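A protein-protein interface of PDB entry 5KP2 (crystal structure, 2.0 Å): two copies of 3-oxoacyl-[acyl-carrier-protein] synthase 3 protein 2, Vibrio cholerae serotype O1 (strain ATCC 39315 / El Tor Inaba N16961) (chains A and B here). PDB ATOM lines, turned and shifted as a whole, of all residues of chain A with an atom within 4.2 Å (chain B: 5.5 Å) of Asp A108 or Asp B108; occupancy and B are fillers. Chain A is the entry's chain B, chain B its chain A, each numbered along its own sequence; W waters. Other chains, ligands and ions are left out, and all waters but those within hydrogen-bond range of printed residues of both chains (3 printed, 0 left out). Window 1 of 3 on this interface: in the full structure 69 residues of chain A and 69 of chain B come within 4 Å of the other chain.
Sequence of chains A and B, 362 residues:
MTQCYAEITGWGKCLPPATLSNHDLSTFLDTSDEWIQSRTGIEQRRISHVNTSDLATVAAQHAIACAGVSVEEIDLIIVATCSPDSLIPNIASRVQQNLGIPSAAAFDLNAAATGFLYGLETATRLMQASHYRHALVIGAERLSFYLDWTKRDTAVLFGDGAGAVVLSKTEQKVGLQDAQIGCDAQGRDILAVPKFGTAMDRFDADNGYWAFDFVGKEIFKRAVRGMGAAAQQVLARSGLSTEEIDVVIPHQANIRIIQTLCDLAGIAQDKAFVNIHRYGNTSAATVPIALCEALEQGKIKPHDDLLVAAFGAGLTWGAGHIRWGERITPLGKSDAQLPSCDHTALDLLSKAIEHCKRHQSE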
ATOM      1  N   VAL A  79      14.819  16.010  16.330  1.00  0.00           N
ATOM      2  CA  VAL A  79      15.121  16.775  15.128  1.00  0.00           C
ATOM      3  C   VAL A  79      16.552  16.445  14.679  1.00  0.00           C
ATOM      4  O   VAL A  79      17.515  16.747  15.371  1.00  0.00           O
ATOM      5  CB  VAL A  79      14.964  18.290  15.334  1.00  0.00           C
ATOM      6  CG1 VAL A  79      15.279  19.019  14.036  1.00  0.00           C
ATOM      7  CG2 VAL A  79      13.554  18.649  15.787  1.00  0.00           C
ATOM      8  N   ASN A  90      18.440  23.731  22.073  1.00  0.00           N
ATOM      9  CA  ASN A  90      18.265  22.941  20.867  1.00  0.00           C
ATOM     10  C   ASN A  90      16.983  23.338  20.089  1.00  0.00           C
ATOM     11  O   ASN A  90      16.091  23.987  20.645  1.00  0.00           O
ATOM     12  CB  ASN A  90      18.320  21.444  21.232  1.00  0.00           C
ATOM     13  CG  ASN A  90      17.104  20.953  22.019  1.00  0.00           C
ATOM     14  OD1 ASN A  90      16.047  21.559  22.011  1.00  0.00           O
ATOM     15  ND2 ASN A  90      17.269  19.851  22.710  1.00  0.00           N
ATOM     16  N   ILE A  91      16.890  22.979  18.811  1.00  0.00           N
ATOM     17  CA  ILE A  91      15.685  23.356  18.034  1.00  0.00           C
ATOM     18  C   ILE A  91      14.506  22.403  18.173  1.00  0.00           C
ATOM     19  O   ILE A  91      13.397  22.793  17.872  1.00  0.00           O
ATOM     20  CB  ILE A  91      15.981  23.675  16.554  1.00  0.00           C
ATOM     21  CG1 ILE A  91      16.497  22.447  15.796  1.00  0.00           C
ATOM     22  CG2 ILE A  91      16.982  24.830  16.469  1.00  0.00           C
ATOM     23  CD1 ILE A  91      16.285  22.575  14.308  1.00  0.00           C
ATOM     24  N   ALA A  92      14.732  21.191  18.688  1.00  0.00           N
ATOM     25  CA  ALA A  92      13.634  20.307  19.067  1.00  0.00           C
ATOM     26  C   ALA A  92      12.711  20.988  20.084  1.00  0.00           C
ATOM     27  O   ALA A  92      11.493  20.901  19.960  1.00  0.00           O
ATOM     28  CB  ALA A  92      14.145  18.991  19.630  1.00  0.00           C
ATOM     29  N   PHE A 107      15.167  16.471  21.710  1.00  0.00           N
ATOM     30  CA  PHE A 107      16.583  16.632  21.404  1.00  0.00           C
ATOM     31  C   PHE A 107      16.909  16.707  19.916  1.00  0.00           C
ATOM     32  O   PHE A 107      16.158  16.227  19.073  1.00  0.00           O
ATOM     33  CB  PHE A 107      17.442  15.575  22.108  1.00  0.00           C
ATOM     34  CG  PHE A 107      17.319  14.177  21.567  1.00  0.00           C
ATOM     35  CD1 PHE A 107      18.186  13.713  20.583  1.00  0.00           C
ATOM     36  CD2 PHE A 107      16.423  13.287  22.126  1.00  0.00           C
ATOM     37  CE1 PHE A 107      18.116  12.397  20.136  1.00  0.00           C
ATOM     38  CE2 PHE A 107      16.331  11.982  21.668  1.00  0.00           C
ATOM     39  CZ  PHE A 107      17.182  11.528  20.689  1.00  0.00           C
ATOM     40  N   ASP A 108      18.038  17.353  19.634  1.00  0.00           N
ATOM     41  CA  ASP A 108      18.568  17.446  18.285  1.00  0.00           C
ATOM     42  C   ASP A 108      19.619  16.351  18.133  1.00  0.00           C
ATOM     43  O   ASP A 108      20.393  16.094  19.057  1.00  0.00           O
ATOM     44  CB  ASP A 108      19.235  18.791  18.019  1.00  0.00           C
ATOM     45  CG  ASP A 108      18.270  19.953  18.056  1.00  0.00           C
ATOM     46  OD1 ASP A 108      17.018  19.733  18.187  1.00  0.00           O
ATOM     47  OD2 ASP A 108      18.761  21.130  17.969  1.00  0.00           O
ATOM     48  N   LEU A 109      19.652  15.750  16.957  1.00  0.00           N
ATOM     49  CA  LEU A 109      20.568  14.682  16.634  1.00  0.00           C
ATOM     50  C   LEU A 109      21.348  15.125  15.401  1.00  0.00           C
ATOM     51  O   LEU A 109      20.754  15.524  14.406  1.00  0.00           O
ATOM     52  CB  LEU A 109      19.770  13.402  16.352  1.00  0.00           C
ATOM     53  CG  LEU A 109      20.558  12.088  16.220  1.00  0.00           C
ATOM     54  CD1 LEU A 109      19.637  10.906  16.492  1.00  0.00           C
ATOM     55  CD2 LEU A 109      21.208  11.930  14.851  1.00  0.00           C
ATOM     56  N   ASN A 110      22.673  15.050  15.466  1.00  0.00           N
ATOM     57  CA  ASN A 110      23.521  15.343  14.325  1.00  0.00           C
ATOM     58  C   ASN A 110      24.307  14.111  13.863  1.00  0.00           C
ATOM     59  O   ASN A 110      25.271  13.679  14.534  1.00  0.00           O
ATOM     60  CB  ASN A 110      24.485  16.489  14.643  1.00  0.00           C
ATOM     61  CG  ASN A 110      25.270  16.948  13.411  1.00  0.00           C
ATOM     62  OD1 ASN A 110      25.066  16.439  12.303  1.00  0.00           O
ATOM     63  ND2 ASN A 110      26.165  17.897  13.598  1.00  0.00           N
ATOM     64  N   ILE B  78      27.871   8.038  21.456  1.00  0.00           N
ATOM     65  CA  ILE B  78      27.029   9.233  21.585  1.00  0.00           C
ATOM     66  C   ILE B  78      27.820  10.302  22.331  1.00  0.00           C
ATOM     67  O   ILE B  78      28.260  10.069  23.461  1.00  0.00           O
ATOM     68  CB  ILE B  78      25.711   8.961  22.363  1.00  0.00           C
ATOM     69  CG1 ILE B  78      24.958   7.790  21.733  1.00  0.00           C
ATOM     70  CG2 ILE B  78      24.856  10.221  22.420  1.00  0.00           C
ATOM     71  CD1 ILE B  78      23.636   7.449  22.415  1.00  0.00           C
ATOM     72  N   VAL B  79      27.964  11.472  21.708  1.00  0.00           N
ATOM     73  CA  VAL B  79      28.524  12.641  22.363  1.00  0.00           C
ATOM     74  C   VAL B  79      27.410  13.662  22.599  1.00  0.00           C
ATOM     75  O   VAL B  79      26.839  14.207  21.657  1.00  0.00           O
ATOM     76  CB  VAL B  79      29.664  13.270  21.547  1.00  0.00           C
ATOM     77  CG1 VAL B  79      30.235  14.468  22.286  1.00  0.00           C
ATOM     78  CG2 VAL B  79      30.774  12.251  21.301  1.00  0.00           C
ATOM     79  N   ALA B  80      27.104  13.887  23.866  1.00  0.00           N
ATOM     80  CA  ALA B  80      26.189  14.927  24.292  1.00  0.00           C
ATOM     81  C   ALA B  80      26.973  16.223  24.487  1.00  0.00           C
ATOM     82  O   ALA B  80      27.911  16.281  25.313  1.00  0.00           O
ATOM     83  CB  ALA B  80      25.504  14.529  25.578  1.00  0.00           C
ATOM     84  N   THR B  81      26.603  17.251  23.733  1.00  0.00           N
ATOM     85  CA  THR B  81      27.310  18.525  23.744  1.00  0.00           C
ATOM     86  C   THR B  81      26.422  19.615  23.150  1.00  0.00           C
ATOM     87  O   THR B  81      25.581  19.338  22.293  1.00  0.00           O
ATOM     88  CB  THR B  81      28.639  18.430  22.942  1.00  0.00           C
ATOM     89  OG1 THR B  81      29.387  19.643  23.063  1.00  0.00           O
ATOM     90  CG2 THR B  81      28.394  18.134  21.460  1.00  0.00           C
ATOM     91  N   PRO B  84      29.961  21.784  20.042  1.00  0.00           N
ATOM     92  CA  PRO B  84      30.807  20.964  19.188  1.00  0.00           C
ATOM     93  C   PRO B  84      31.779  21.797  18.348  1.00  0.00           C
ATOM     94  O   PRO B  84      31.436  22.921  17.944  1.00  0.00           O
ATOM     95  CB  PRO B  84      29.798  20.256  18.292  1.00  0.00           C
ATOM     96  CG  PRO B  84      28.680  21.232  18.158  1.00  0.00           C
ATOM     97  CD  PRO B  84      28.584  21.900  19.503  1.00  0.00           C
ATOM     98  N   SER B  86      32.647  21.376  15.373  1.00  0.00           N
ATOM     99  CA  SER B  86      32.034  21.559  14.072  1.00  0.00           C
ATOM    100  C   SER B  86      30.652  20.914  14.057  1.00  0.00           C
ATOM    101  O   SER B  86      30.351  20.034  14.867  1.00  0.00           O
ATOM    102  CB  SER B  86      32.912  20.937  12.974  1.00  0.00           C
ATOM    103  OG  SER B  86      32.951  19.520  13.104  1.00  0.00           O
ATOM    104  N   PRO B  89      31.540  17.537   9.842  1.00  0.00           N
ATOM    105  CA  PRO B  89      30.724  16.475  10.400  1.00  0.00           C
ATOM    106  C   PRO B  89      30.575  16.656  11.900  1.00  0.00           C
ATOM    107  O   PRO B  89      31.080  17.624  12.481  1.00  0.00           O
ATOM    108  CB  PRO B  89      31.540  15.191  10.102  1.00  0.00           C
ATOM    109  CG  PRO B  89      32.814  15.641   9.449  1.00  0.00           C
ATOM    110  CD  PRO B  89      32.948  17.102   9.723  1.00  0.00           C
ATOM    111  N   ASN B  90      29.897  15.701  12.517  1.00  0.00           N
ATOM    112  CA  ASN B  90      29.687  15.691  13.956  1.00  0.00           C
ATOM    113  C   ASN B  90      30.979  15.352  14.727  1.00  0.00           C
ATOM    114  O   ASN B  90      31.939  14.817  14.151  1.00  0.00           O
ATOM    115  CB  ASN B  90      28.497  14.761  14.287  1.00  0.00           C
ATOM    116  CG  ASN B  90      28.799  13.285  14.075  1.00  0.00           C
ATOM    117  OD1 ASN B  90      29.940  12.862  14.044  1.00  0.00           O
ATOM    118  ND2 ASN B  90      27.763  12.503  13.925  1.00  0.00           N
ATOM    119  N   ILE B  91      31.044  15.671  16.020  1.00  0.00           N
ATOM    120  CA  ILE B  91      32.275  15.360  16.790  1.00  0.00           C
ATOM    121  C   ILE B  91      32.351  13.937  17.335  1.00  0.00           C
ATOM    122  O   ILE B  91      33.430  13.492  17.689  1.00  0.00           O
ATOM    123  CB  ILE B  91      32.594  16.396  17.892  1.00  0.00           C
ATOM    124  CG1 ILE B  91      31.529  16.417  18.984  1.00  0.00           C
ATOM    125  CG2 ILE B  91      32.781  17.777  17.265  1.00  0.00           C
ATOM    126  CD1 ILE B  91      32.060  16.994  20.281  1.00  0.00           C
ATOM    127  N   ALA B  92      31.230  13.213  17.378  1.00  0.00           N
ATOM    128  CA  ALA B  92      31.259  11.782  17.682  1.00  0.00           C
ATOM    129  C   ALA B  92      32.171  11.057  16.698  1.00  0.00           C
ATOM    130  O   ALA B  92      32.932  10.183  17.101  1.00  0.00           O
ATOM    131  CB  ALA B  92      29.859  11.173  17.650  1.00  0.00           C
ATOM    132  N   SER B  93      32.074  11.413  15.412  1.00  0.00           N
ATOM    133  CA  SER B  93      32.927  10.824  14.384  1.00  0.00           C
ATOM    134  C   SER B  93      34.407  11.168  14.585  1.00  0.00           C
ATOM    135  O   SER B  93      35.264  10.398  14.177  1.00  0.00           O
ATOM    136  CB  SER B  93      32.466  11.205  12.956  1.00  0.00           C
ATOM    137  OG  SER B  93      32.543  12.599  12.702  1.00  0.00           O
ATOM    138  N   ALA B 106      27.768   6.669  15.239  1.00  0.00           N
ATOM    139  CA  ALA B 106      28.366   7.821  15.894  1.00  0.00           C
ATOM    140  C   ALA B 106      27.498   9.052  15.668  1.00  0.00           C
ATOM    141  O   ALA B 106      27.360   9.501  14.537  1.00  0.00           O
ATOM    142  CB  ALA B 106      29.779   8.068  15.359  1.00  0.00           C
ATOM    143  N   PHE B 107      26.941   9.608  16.742  1.00  0.00           N
ATOM    144  CA  PHE B 107      26.184  10.841  16.623  1.00  0.00           C
ATOM    145  C   PHE B 107      26.313  11.771  17.817  1.00  0.00           C
ATOM    146  O   PHE B 107      26.636  11.339  18.934  1.00  0.00           O
ATOM    147  CB  PHE B 107      24.714  10.565  16.298  1.00  0.00           C
ATOM    148  CG  PHE B 107      23.916   9.935  17.407  1.00  0.00           C
ATOM    149  CD1 PHE B 107      23.891   8.556  17.574  1.00  0.00           C
ATOM    150  CD2 PHE B 107      23.097  10.719  18.210  1.00  0.00           C
ATOM    151  CE1 PHE B 107      23.091   7.975  18.560  1.00  0.00           C
ATOM    152  CE2 PHE B 107      22.303  10.153  19.191  1.00  0.00           C
ATOM    153  CZ  PHE B 107      22.298   8.784  19.376  1.00  0.00           C
ATOM    154  N   ASP B 108      26.075  13.055  17.546  1.00  0.00           N
ATOM    155  CA  ASP B 108      26.050  14.067  18.583  1.00  0.00           C
ATOM    156  C   ASP B 108      24.607  14.289  18.990  1.00  0.00           C
ATOM    157  O   ASP B 108      23.712  14.294  18.145  1.00  0.00           O
ATOM    158  CB  ASP B 108      26.622  15.392  18.087  1.00  0.00           C
ATOM    159  CG  ASP B 108      28.097  15.316  17.740  1.00  0.00           C
ATOM    160  OD1 ASP B 108      28.745  14.251  17.977  1.00  0.00           O
ATOM    161  OD2 ASP B 108      28.633  16.337  17.207  1.00  0.00           O
ATOM    162  N   LEU B 109      24.394  14.489  20.279  1.00  0.00           N
ATOM    163  CA  LEU B 109      23.070  14.697  20.838  1.00  0.00           C
ATOM    164  C   LEU B 109      23.095  16.028  21.568  1.00  0.00           C
ATOM    165  O   LEU B 109      23.987  16.268  22.388  1.00  0.00           O
ATOM    166  CB  LEU B 109      22.736  13.563  21.808  1.00  0.00           C
ATOM    167  CG  LEU B 109      21.299  13.474  22.353  1.00  0.00           C
ATOM    168  CD1 LEU B 109      21.010  12.056  22.832  1.00  0.00           C
ATOM    169  CD2 LEU B 109      21.032  14.445  23.486  1.00  0.00           C
ATOM    170  N   ASN B 110      22.133  16.897  21.268  1.00  0.00           N
ATOM    171  CA  ASN B 110      22.006  18.168  21.953  1.00  0.00           C
ATOM    172  C   ASN B 110      20.695  18.259  22.739  1.00  0.00           C
ATOM    173  O   ASN B 110      19.605  18.423  22.148  1.00  0.00           O
ATOM    174  CB  ASN B 110      22.106  19.326  20.967  1.00  0.00           C
ATOM    175  CG  ASN B 110      22.149  20.683  21.668  1.00  0.00           C
ATOM    176  OD1 ASN B 110      22.147  20.763  22.902  1.00  0.00           O
ATOM    177  ND2 ASN B 110      22.184  21.750  20.889  1.00  0.00           N
ATOM    178  N   ALA B 111      20.819  18.159  24.065  1.00  0.00           N
ATOM    179  CA  ALA B 111      19.727  18.489  25.001  1.00  0.00           C
ATOM    180  C   ALA B 111      20.262  19.292  26.187  1.00  0.00           C
ATOM    181  O   ALA B 111      19.807  19.118  27.329  1.00  0.00           O
ATOM    182  CB  ALA B 111      19.033  17.233  25.482  1.00  0.00           C
HETATM  183  O   HOH W   1      21.443  22.316  18.256  1.00  0.00           O
HETATM  184  O   HOH W   2      23.068  17.434  17.946  1.00  0.00           O
HETATM  185  O   HOH W   3      27.860  18.663  15.881  1.00  0.00           O
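Asp A108 touches three residues of chain B.
Of chain A, only Asp A108 (3.9 Å), Leu A109 (3.5 Å) and Asn A110 (3.0 Å) come within 4 Å of Asp B108.
Of the printed residues of chain A, Ala B111 touches Asn A90 (3.6 Å).
Of the printed residues of chain B, Phe A107 touches Leu B109 and Asn B110.
Printed residues of chain B within 4 Å of Asn A110: Asn B90 (2.8 Å), Phe B107 (3.6 Å) and Asp B108 (3.0 Å).
Of the printed residues of chain A, Leu B109 touches Phe A107 and Asp A108.
Printed residues of chain A within 4 Å of Asn B110: Asn A90, Phe A107 and Asp A108.
Ala B106 touches none of the printed residues of chain A.
The nearest printed residue of chain A that does not touch Asp B108 is Phe A107 (6.1 Å).
The backbone NH of Asn B110 lies within hydrogen-bond range of the backbone carbonyl oxygen of Asp A108 (2.9 Å).
ND2 of Asn B90 lies within hydrogen-bond range of O of Asn A110 (2.8 Å).
The backbone NH (N) of Asn A110 is in hydrogen-bond range of the backbone carbonyl oxygen (O) of Asp B108, at 3.0 Å.
O of Asn B110 lies within hydrogen-bond range of ND2 of Asn A90 (2.8 Å).
The backbone NH (N) of Ala A92 lies within hydrogen-bond range of the side-chain carboxylate (OD1) of Asp A108.
The backbone NH (N) of Leu B109 sits at hydrogen-bond distance from the backbone carbonyl oxygen (O) of Val B79 (2.8 Å).
The backbone NH (N) of Ala B92 sits at hydrogen-bond distance from the side-chain carboxylate (OD1) of Asp B108, at 2.8 Å.
The side-chain hydroxyl of Ser B93 lies within hydrogen-bond range of the backbone carbonyl oxygen of Asn B90, 2.7 Å away.
The backbone NH (N) of Ile A91 lies within hydrogen-bond range of the side-chain carboxylate (OD2) of Asp A108 (2.8 Å).
The backbone NH (N) of Thr B81 sits at hydrogen-bond distance from the backbone carbonyl oxygen (O) of Leu B109, at 3.1 Å.
Hydrophobic or aromatic side chains of chain A within 4 Å of the printed part of chain B: Phe A107 and Leu A109.
Hydrophobic or aromatic side chains of chain B that line the printed part of chain A: Phe B107 and Leu B109.
Among the printed residues, no Asp or Glu carboxylate lies within 4 Å of a Lys or Arg side-chain nitrogen of the other chain.
ND2 of Asn A90 touches CA of Ala B111, 3.6 Å away.
Leu B109 touches Phe A107 (CG to CD1, 3.6 Å).
Asn B110 touches Phe A107 (O to CB, 3.6 Å).
O of Asp A108 touches O of Asp B108, 3.9 Å away.
Leu B109 touches Asp A108 (CA to O, 3.5 Å).
Leu A109 touches Phe B107.
CA of Leu A109 touches O of Asp B108 (3.5 Å).
Asn A110 touches Phe B107 (O to CB, 3.6 Å).
Water W3 lies within hydrogen-bond range of the side-chain carboxylate (OD2) of Asp B108 (2.8 Å), the side-chain amide nitrogen (ND2) of Asn A110 (2.9 Å) and the backbone carbonyl oxygen (O) of Ser B86 (3.0 Å).
Water W1 lies within hydrogen-bond range of ND2 of Asn B110 and OD2 of Asp A108.
Water W2 lies within hydrogen-bond range of O of Asp A108, O of Asp B108, N of Asn A110 and N of Asn B110.
Phe A107 touches Leu B109, and with the chains exchanged Leu A109 touches Phe B107.
Phe A107 touches Asn B110, and with the chains exchanged Asn A110 touches Phe B107.
Asp A108 touches its own counterpart, Asp B108.
Asp A108 touches Leu B109, and with the chains exchanged Leu A109 touches Asp B108.
8 positions are printed for both chains.
Of the 12 pairs that touch across the chains among the printed residues, 11 have their exchanged pair printed and touching as well.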
